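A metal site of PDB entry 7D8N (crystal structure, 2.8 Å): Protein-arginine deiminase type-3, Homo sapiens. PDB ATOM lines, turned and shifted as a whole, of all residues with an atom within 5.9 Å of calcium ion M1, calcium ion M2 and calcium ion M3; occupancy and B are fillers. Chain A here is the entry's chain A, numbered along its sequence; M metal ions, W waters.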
ATOM      1  N   ASN A 153      34.188   9.113 -24.692  1.00  0.00           N
ATOM      2  CA  ASN A 153      32.816   9.208 -24.203  1.00  0.00           C
ATOM      3  C   ASN A 153      32.819   9.515 -22.705  1.00  0.00           C
ATOM      4  O   ASN A 153      32.481   8.694 -21.853  1.00  0.00           O
ATOM      5  CB  ASN A 153      32.072   7.909 -24.507  1.00  0.00           C
ATOM      6  CG  ASN A 153      30.596   8.001 -24.225  1.00  0.00           C
ATOM      7  OD1 ASN A 153      30.067   9.090 -23.971  1.00  0.00           O
ATOM      8  ND2 ASN A 153      29.908   6.872 -24.265  1.00  0.00           N
ATOM      9  N   CYS A 154      33.203  10.758 -22.391  1.00  0.00           N
ATOM     10  CA  CYS A 154      33.457  11.179 -21.022  1.00  0.00           C
ATOM     11  C   CYS A 154      32.434  12.197 -20.511  1.00  0.00           C
ATOM     12  O   CYS A 154      32.775  13.018 -19.655  1.00  0.00           O
ATOM     13  CB  CYS A 154      34.870  11.757 -20.912  1.00  0.00           C
ATOM     14  SG  CYS A 154      35.182  13.128 -22.057  1.00  0.00           S
ATOM     15  N   ASP A 155      31.191  12.165 -21.001  1.00  0.00           N
ATOM     16  CA  ASP A 155      30.284  13.277 -20.777  1.00  0.00           C
ATOM     17  C   ASP A 155      29.048  12.978 -19.936  1.00  0.00           C
ATOM     18  O   ASP A 155      28.316  13.916 -19.623  1.00  0.00           O
ATOM     19  CB  ASP A 155      29.837  13.886 -22.120  1.00  0.00           C
ATOM     20  CG  ASP A 155      28.887  12.993 -22.893  1.00  0.00           C
ATOM     21  OD1 ASP A 155      29.117  11.764 -22.931  1.00  0.00           O
ATOM     22  OD2 ASP A 155      27.920  13.525 -23.470  1.00  0.00           O
ATOM     23  N   ARG A 156      28.795  11.738 -19.535  1.00  0.00           N
ATOM     24  CA  ARG A 156      27.704  11.421 -18.597  1.00  0.00           C
ATOM     25  C   ARG A 156      26.341  11.879 -19.131  1.00  0.00           C
ATOM     26  O   ARG A 156      25.720  12.809 -18.624  1.00  0.00           O
ATOM     27  CB  ARG A 156      27.982  12.027 -17.212  1.00  0.00           C
ATOM     28  CG  ARG A 156      26.977  11.619 -16.146  1.00  0.00           C
ATOM     29  CD  ARG A 156      26.863  12.689 -15.093  1.00  0.00           C
ATOM     30  NE  ARG A 156      27.747  12.438 -13.963  1.00  0.00           N
ATOM     31  CZ  ARG A 156      28.094  13.357 -13.066  1.00  0.00           C
ATOM     32  NH1 ARG A 156      27.640  14.590 -13.174  1.00  0.00           N
ATOM     33  NH2 ARG A 156      28.899  13.038 -12.069  1.00  0.00           N
ATOM     34  N   ASP A 157      25.904  11.204 -20.190  1.00  0.00           N
ATOM     35  CA  ASP A 157      24.576  11.464 -20.736  1.00  0.00           C
ATOM     36  C   ASP A 157      23.471  10.836 -19.908  1.00  0.00           C
ATOM     37  O   ASP A 157      22.325  11.305 -19.956  1.00  0.00           O
ATOM     38  CB  ASP A 157      24.464  10.930 -22.173  1.00  0.00           C
ATOM     39  CG  ASP A 157      25.204  11.798 -23.168  1.00  0.00           C
ATOM     40  OD1 ASP A 157      25.181  13.041 -23.021  1.00  0.00           O
ATOM     41  OD2 ASP A 157      25.801  11.230 -24.103  1.00  0.00           O
ATOM     42  N   GLN A 164      30.704   8.920 -15.346  1.00  0.00           N
ATOM     43  CA  GLN A 164      30.864   9.042 -16.789  1.00  0.00           C
ATOM     44  C   GLN A 164      30.313   7.817 -17.499  1.00  0.00           C
ATOM     45  O   GLN A 164      30.239   6.714 -16.945  1.00  0.00           O
ATOM     46  CB  GLN A 164      32.329   9.265 -17.142  1.00  0.00           C
ATOM     47  CG  GLN A 164      32.831  10.660 -16.789  1.00  0.00           C
ATOM     48  CD  GLN A 164      34.338  10.711 -16.611  1.00  0.00           C
ATOM     49  OE1 GLN A 164      35.046  11.357 -17.395  1.00  0.00           O
ATOM     50  NE2 GLN A 164      34.838  10.057 -15.573  1.00  0.00           N
ATOM     51  N   ASP A 165      29.921   8.012 -18.755  1.00  0.00           N
ATOM     52  CA  ASP A 165      29.237   6.958 -19.502  1.00  0.00           C
ATOM     53  C   ASP A 165      30.147   5.805 -19.871  1.00  0.00           C
ATOM     54  O   ASP A 165      29.659   4.695 -20.083  1.00  0.00           O
ATOM     55  CB  ASP A 165      28.592   7.533 -20.771  1.00  0.00           C
ATOM     56  CG  ASP A 165      27.486   8.518 -20.461  1.00  0.00           C
ATOM     57  OD1 ASP A 165      26.879   8.418 -19.374  1.00  0.00           O
ATOM     58  OD2 ASP A 165      27.212   9.395 -21.312  1.00  0.00           O
ATOM     59  N   ASN A 166      31.455   6.034 -19.965  1.00  0.00           N
ATOM     60  CA  ASN A 166      32.390   5.013 -20.402  1.00  0.00           C
ATOM     61  C   ASN A 166      33.030   4.245 -19.241  1.00  0.00           C
ATOM     62  O   ASN A 166      34.093   3.645 -19.420  1.00  0.00           O
ATOM     63  CB  ASN A 166      33.473   5.629 -21.289  1.00  0.00           C
ATOM     64  CG  ASN A 166      34.287   6.694 -20.583  1.00  0.00           C
ATOM     65  OD1 ASN A 166      34.070   6.983 -19.404  1.00  0.00           O
ATOM     66  ND2 ASN A 166      35.230   7.284 -21.301  1.00  0.00           N
ATOM     67  N   CYS A 167      32.419   4.258 -18.062  1.00  0.00           N
ATOM     68  CA  CYS A 167      32.973   3.534 -16.929  1.00  0.00           C
ATOM     69  C   CYS A 167      32.525   2.081 -16.868  1.00  0.00           C
ATOM     70  O   CYS A 167      33.268   1.241 -16.374  1.00  0.00           O
ATOM     71  CB  CYS A 167      32.610   4.244 -15.621  1.00  0.00           C
ATOM     72  SG  CYS A 167      33.334   5.884 -15.468  1.00  0.00           S
ATOM     73  N   ASP A 168      31.324   1.781 -17.343  1.00  0.00           N
ATOM     74  CA  ASP A 168      30.807   0.426 -17.325  1.00  0.00           C
ATOM     75  C   ASP A 168      31.043  -0.232 -18.689  1.00  0.00           C
ATOM     76  O   ASP A 168      31.768   0.281 -19.544  1.00  0.00           O
ATOM     77  CB  ASP A 168      29.335   0.418 -16.928  1.00  0.00           C
ATOM     78  CG  ASP A 168      28.495   1.383 -17.746  1.00  0.00           C
ATOM     79  OD1 ASP A 168      28.988   1.862 -18.793  1.00  0.00           O
ATOM     80  OD2 ASP A 168      27.350   1.647 -17.344  1.00  0.00           O
ATOM     81  N   GLN A 169      30.426  -1.396 -18.881  1.00  0.00           N
ATOM     82  CA  GLN A 169      30.469  -2.118 -20.147  1.00  0.00           C
ATOM     83  C   GLN A 169      29.070  -2.284 -20.725  1.00  0.00           C
ATOM     84  O   GLN A 169      28.745  -3.318 -21.321  1.00  0.00           O
ATOM     85  CB  GLN A 169      31.153  -3.476 -19.978  1.00  0.00           C
ATOM     86  CG  GLN A 169      32.603  -3.385 -19.549  1.00  0.00           C
ATOM     87  CD  GLN A 169      33.293  -4.733 -19.561  1.00  0.00           C
ATOM     88  OE1 GLN A 169      32.771  -5.708 -20.096  1.00  0.00           O
ATOM     89  NE2 GLN A 169      34.489  -4.797 -18.974  1.00  0.00           N
ATOM     90  N   HIS A 170      28.216  -1.276 -20.545  1.00  0.00           N
ATOM     91  CA  HIS A 170      26.845  -1.331 -21.024  1.00  0.00           C
ATOM     92  C   HIS A 170      26.455   0.026 -21.582  1.00  0.00           C
ATOM     93  O   HIS A 170      27.070   1.050 -21.275  1.00  0.00           O
ATOM     94  CB  HIS A 170      25.861  -1.733 -19.922  1.00  0.00           C
ATOM     95  CG  HIS A 170      26.269  -2.954 -19.153  1.00  0.00           C
ATOM     96  ND1 HIS A 170      25.883  -4.232 -19.525  1.00  0.00           N
ATOM     97  CD2 HIS A 170      27.018  -3.099 -18.042  1.00  0.00           C
ATOM     98  CE1 HIS A 170      26.386  -5.100 -18.672  1.00  0.00           C
ATOM     99  NE2 HIS A 170      27.072  -4.441 -17.758  1.00  0.00           N
ATOM    100  N   VAL A 171      25.430   0.020 -22.429  1.00  0.00           N
ATOM    101  CA  VAL A 171      24.762   1.232 -22.877  1.00  0.00           C
ATOM    102  C   VAL A 171      23.498   1.389 -22.043  1.00  0.00           C
ATOM    103  O   VAL A 171      22.636   0.498 -22.029  1.00  0.00           O
ATOM    104  CB  VAL A 171      24.435   1.167 -24.384  1.00  0.00           C
ATOM    105  CG1 VAL A 171      23.604   2.371 -24.797  1.00  0.00           C
ATOM    106  CG2 VAL A 171      25.718   1.093 -25.199  1.00  0.00           C
ATOM    107  N   HIS A 172      23.390   2.505 -21.334  1.00  0.00           N
ATOM    108  CA  HIS A 172      22.273   2.748 -20.436  1.00  0.00           C
ATOM    109  C   HIS A 172      21.373   3.894 -20.875  1.00  0.00           C
ATOM    110  O   HIS A 172      20.423   4.220 -20.160  1.00  0.00           O
ATOM    111  CB  HIS A 172      22.787   3.003 -19.014  1.00  0.00           C
ATOM    112  CG  HIS A 172      23.275   1.774 -18.316  1.00  0.00           C
ATOM    113  ND1 HIS A 172      22.799   0.508 -18.626  1.00  0.00           N
ATOM    114  CD2 HIS A 172      24.185   1.599 -17.336  1.00  0.00           C
ATOM    115  CE1 HIS A 172      23.404  -0.387 -17.857  1.00  0.00           C
ATOM    116  NE2 HIS A 172      24.248   0.246 -17.066  1.00  0.00           N
ATOM    117  N   GLN A 175      20.855   8.230 -26.061  1.00  0.00           N
ATOM    118  CA  GLN A 175      21.599   9.424 -26.445  1.00  0.00           C
ATOM    119  C   GLN A 175      23.108   9.215 -26.349  1.00  0.00           C
ATOM    120  O   GLN A 175      23.863   9.958 -26.972  1.00  0.00           O
ATOM    121  CB  GLN A 175      21.160  10.631 -25.597  1.00  0.00           C
ATOM    122  CG  GLN A 175      21.166  10.403 -24.090  1.00  0.00           C
ATOM    123  CD  GLN A 175      19.847   9.873 -23.566  1.00  0.00           C
ATOM    124  OE1 GLN A 175      19.382   8.805 -23.986  1.00  0.00           O
ATOM    125  NE2 GLN A 175      19.235  10.613 -22.656  1.00  0.00           N
ATOM    126  N   ASP A 176      23.550   8.221 -25.576  1.00  0.00           N
ATOM    127  CA  ASP A 176      24.981   7.940 -25.459  1.00  0.00           C
ATOM    128  C   ASP A 176      25.587   7.547 -26.802  1.00  0.00           C
ATOM    129  O   ASP A 176      26.749   7.845 -27.057  1.00  0.00           O
ATOM    130  CB  ASP A 176      25.210   6.838 -24.430  1.00  0.00           C
ATOM    131  CG  ASP A 176      26.656   6.772 -23.970  1.00  0.00           C
ATOM    132  OD1 ASP A 176      27.398   7.739 -24.203  1.00  0.00           O
ATOM    133  OD2 ASP A 176      27.044   5.741 -23.378  1.00  0.00           O
ATOM    134  N   GLU A 178      25.148   8.836 -29.576  1.00  0.00           N
ATOM    135  CA  GLU A 178      25.478  10.010 -30.376  1.00  0.00           C
ATOM    136  C   GLU A 178      26.948  10.394 -30.243  1.00  0.00           C
ATOM    137  O   GLU A 178      27.462  11.099 -31.128  1.00  0.00           O
ATOM    138  CB  GLU A 178      24.593  11.185 -29.968  1.00  0.00           C
ATOM    139  CG  GLU A 178      23.105  10.920 -30.157  1.00  0.00           C
ATOM    140  CD  GLU A 178      22.247  12.123 -29.767  1.00  0.00           C
ATOM    141  OE1 GLU A 178      21.019  11.929 -29.612  1.00  0.00           O
ATOM    142  OE2 GLU A 178      22.797  13.233 -29.614  1.00  0.00           O
ATOM    143  N   ASP A 179      27.627   9.972 -29.175  1.00  0.00           N
ATOM    144  CA  ASP A 179      29.047  10.240 -28.986  1.00  0.00           C
ATOM    145  C   ASP A 179      29.946   9.216 -29.674  1.00  0.00           C
ATOM    146  O   ASP A 179      31.110   9.524 -29.949  1.00  0.00           O
ATOM    147  CB  ASP A 179      29.407  10.265 -27.501  1.00  0.00           C
ATOM    148  CG  ASP A 179      28.553  11.230 -26.702  1.00  0.00           C
ATOM    149  OD1 ASP A 179      28.382  12.383 -27.135  1.00  0.00           O
ATOM    150  OD2 ASP A 179      28.062  10.832 -25.619  1.00  0.00           O
ATOM    151  N   PHE A 214      30.752  -2.120 -28.989  1.00  0.00           N
ATOM    152  CA  PHE A 214      29.484  -2.825 -28.786  1.00  0.00           C
ATOM    153  C   PHE A 214      28.941  -3.259 -30.135  1.00  0.00           C
ATOM    154  O   PHE A 214      28.850  -2.454 -31.060  1.00  0.00           O
ATOM    155  CB  PHE A 214      28.455  -1.932 -28.092  1.00  0.00           C
ATOM    156  CG  PHE A 214      28.923  -1.357 -26.779  1.00  0.00           C
ATOM    157  CD1 PHE A 214      29.623  -0.169 -26.748  1.00  0.00           C
ATOM    158  CD2 PHE A 214      28.657  -2.015 -25.594  1.00  0.00           C
ATOM    159  CE1 PHE A 214      30.052   0.361 -25.548  1.00  0.00           C
ATOM    160  CE2 PHE A 214      29.078  -1.497 -24.391  1.00  0.00           C
ATOM    161  CZ  PHE A 214      29.777  -0.301 -24.366  1.00  0.00           C
ATOM    162  N   GLU A 252      33.738   3.456 -28.713  1.00  0.00           N
ATOM    163  CA  GLU A 252      33.626   4.384 -27.597  1.00  0.00           C
ATOM    164  C   GLU A 252      35.016   4.568 -27.010  1.00  0.00           C
ATOM    165  O   GLU A 252      35.634   3.597 -26.560  1.00  0.00           O
ATOM    166  CB  GLU A 252      32.651   3.831 -26.556  1.00  0.00           C
ATOM    167  CG  GLU A 252      32.742   4.446 -25.190  1.00  0.00           C
ATOM    168  CD  GLU A 252      31.896   3.694 -24.177  1.00  0.00           C
ATOM    169  OE1 GLU A 252      32.213   2.514 -23.900  1.00  0.00           O
ATOM    170  OE2 GLU A 252      30.909   4.261 -23.686  1.00  0.00           O
ATOM    171  N   LYS A 362      29.883  14.919 -33.749  1.00  0.00           N
ATOM    172  CA  LYS A 362      29.511  15.536 -32.475  1.00  0.00           C
ATOM    173  C   LYS A 362      30.663  16.361 -31.918  1.00  0.00           C
ATOM    174  O   LYS A 362      31.831  15.991 -32.039  1.00  0.00           O
ATOM    175  CB  LYS A 362      29.084  14.473 -31.457  1.00  0.00           C
ATOM    176  CG  LYS A 362      28.607  15.043 -30.141  1.00  0.00           C
ATOM    177  CD  LYS A 362      27.587  14.128 -29.491  1.00  0.00           C
ATOM    178  CE  LYS A 362      26.176  14.558 -29.828  1.00  0.00           C
ATOM    179  NZ  LYS A 362      25.940  15.979 -29.455  1.00  0.00           N
ATOM    180  N   LEU A 364      31.831  18.179 -28.253  1.00  0.00           N
ATOM    181  CA  LEU A 364      31.586  18.168 -26.817  1.00  0.00           C
ATOM    182  C   LEU A 364      32.491  19.188 -26.135  1.00  0.00           C
ATOM    183  O   LEU A 364      33.726  19.058 -26.228  1.00  0.00           O
ATOM    184  CB  LEU A 364      31.833  16.780 -26.224  1.00  0.00           C
ATOM    185  CG  LEU A 364      31.032  15.589 -26.735  1.00  0.00           C
ATOM    186  CD1 LEU A 364      31.446  14.355 -25.967  1.00  0.00           C
ATOM    187  CD2 LEU A 364      29.544  15.835 -26.614  1.00  0.00           C
ATOM    188  N   PRO A 387      25.178  15.993 -19.506  1.00  0.00           N
ATOM    189  CA  PRO A 387      24.950  15.537 -20.876  1.00  0.00           C
ATOM    190  C   PRO A 387      25.564  16.493 -21.899  1.00  0.00           C
ATOM    191  O   PRO A 387      25.374  17.712 -21.831  1.00  0.00           O
ATOM    192  CB  PRO A 387      23.417  15.500 -20.984  1.00  0.00           C
ATOM    193  CG  PRO A 387      22.922  16.364 -19.878  1.00  0.00           C
ATOM    194  CD  PRO A 387      23.914  16.197 -18.774  1.00  0.00           C
ATOM    195  N   ASP A 388      26.337  15.920 -22.823  1.00  0.00           N
ATOM    196  CA  ASP A 388      27.066  16.684 -23.831  1.00  0.00           C
ATOM    197  C   ASP A 388      28.025  17.701 -23.212  1.00  0.00           C
ATOM    198  O   ASP A 388      28.236  18.796 -23.736  1.00  0.00           O
ATOM    199  CB  ASP A 388      26.110  17.376 -24.805  1.00  0.00           C
ATOM    200  CG  ASP A 388      25.732  16.490 -25.975  1.00  0.00           C
ATOM    201  OD1 ASP A 388      25.846  15.254 -25.843  1.00  0.00           O
ATOM    202  OD2 ASP A 388      25.338  17.028 -27.031  1.00  0.00           O
ATOM    203  N   PHE A 389      28.611  17.327 -22.083  1.00  0.00           N
ATOM    204  CA  PHE A 389      29.661  18.136 -21.464  1.00  0.00           C
ATOM    205  C   PHE A 389      30.589  17.161 -20.738  1.00  0.00           C
ATOM    206  O   PHE A 389      30.212  16.615 -19.699  1.00  0.00           O
ATOM    207  CB  PHE A 389      29.080  19.178 -20.523  1.00  0.00           C
ATOM    208  CG  PHE A 389      29.865  20.461 -20.485  1.00  0.00           C
ATOM    209  CD1 PHE A 389      31.253  20.458 -20.513  1.00  0.00           C
ATOM    210  CD2 PHE A 389      29.213  21.685 -20.441  1.00  0.00           C
ATOM    211  CE1 PHE A 389      31.973  21.646 -20.470  1.00  0.00           C
ATOM    212  CE2 PHE A 389      29.927  22.872 -20.415  1.00  0.00           C
ATOM    213  CZ  PHE A 389      31.309  22.850 -20.433  1.00  0.00           C
HETATM  214 CA    CA M   1      27.882   3.126 -20.488  1.00  0.00          CA
HETATM  215 CA    CA M   2      27.905   9.889 -23.495  1.00  0.00          CA
HETATM  216 CA    CA M   3      26.544  12.990 -25.404  1.00  0.00          CA
HETATM  217  O   HOH W   1      28.622   3.745 -22.844  1.00  0.00           O
HETATM  218  O   HOH W   2      24.415  12.338 -26.788  1.00  0.00           O
HETATM  219  O   HOH W   3      29.746   2.140 -21.477  1.00  0.00           O
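The side-chain amide nitrogen (ND2) of Asn 153 lies within hydrogen-bond range of the side-chain carboxylate (OE2) of Glu 252 (2.9 Å).
The side-chain amino group (NZ) of Lys 362 is in salt-bridge range of the side-chain carboxylate (OD2) of Asp 388 (2.7 Å).
A ring nitrogen (NE2) of His 172 lies close to the side-chain carboxylate (OD2) of Asp 168, at 3.4 Å.
The backbone carbonyl oxygen (O) of Asn 153 sits close to the side-chain amide nitrogen (ND2) of Asn 166, at 3.1 Å.
The side-chain carboxylate (OD2) of Asp 165 sits close to the backbone NH (N) of Arg 156 (3.3 Å).
Four residues have an atom within 4 Å of calcium ion M1: Asp 165, Asp 168, His 170 and Asp 176.
Along chain A the residues within 4 Å of calcium ion M1 span positions 165 to 176.
Of the 25 residues printed, 6 come within 4 Å of calcium ion M2.
Within 4 Å of calcium ion M3: Asp 155, Asp 157, Asp 179 and Asp 388.
The nearest printed residue that does not touch calcium ion M3 is Leu 364 (4.3 Å).
Water W3 binds calcium ion M1, 2.3 Å away.
The backbone carbonyl oxygen (O) of His 170 binds calcium ion M1 (2.4 Å).
OD1 of Asp 168 is bound to calcium ion M1 (2.4 Å).
The backbone carbonyl oxygen (O) of Asp 165 is bound to calcium ion M1.
Water W1 binds calcium ion M1 (2.5 Å).
Calcium ion M1 has five donor atoms within binding distance.
OD1 of Asp 155 binds calcium ion M2, at 2.3 Å.
OD1 of Asp 176 is bound to calcium ion M2 (2.3 Å).
Calcium ion M2 is bound by OD2 of Asp 179 (2.3 Å).
Calcium ion M2 is bound by OD2 of Asp 165, 2.3 Å away.
Calcium ion M2 is bound by the side-chain amide oxygen (OD1) of Asn 153.
OD2 of Asp 157 binds calcium ion M2.
Calcium ion M2 has six donor atoms within binding distance.
Calcium ion M3 is bound by the side-chain carboxylate (OD2) of Asp 157 (2.3 Å), the side-chain carboxylate (OD1) of Asp 388 (2.4 Å), the side-chain carboxylate (OD2) of Asp 155 (2.4 Å), the side-chain carboxylate (OD1) of Asp 179 (2.6 Å), water W2 (2.6 Å), the side-chain carboxylate (OD2) of Asp 179 (2.6 Å) and the side-chain carboxylate (OD1) of Asp 157 (2.7 Å).
Calcium ion M3 has seven donor atoms within binding distance.
Water W3 lies within hydrogen-bond range of OE2 of Glu 252 (3.3 Å) and O of Asp 168 (3.4 Å).
Water W1 bridges the side-chain carboxylate of Glu 252 (2.5 Å) and the side-chain carboxylate of Asp 176 (2.6 Å).
Water W2 lies within hydrogen-bond range of the backbone carbonyl oxygen of Gln 175 and the side-chain carboxylate of Glu 178.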
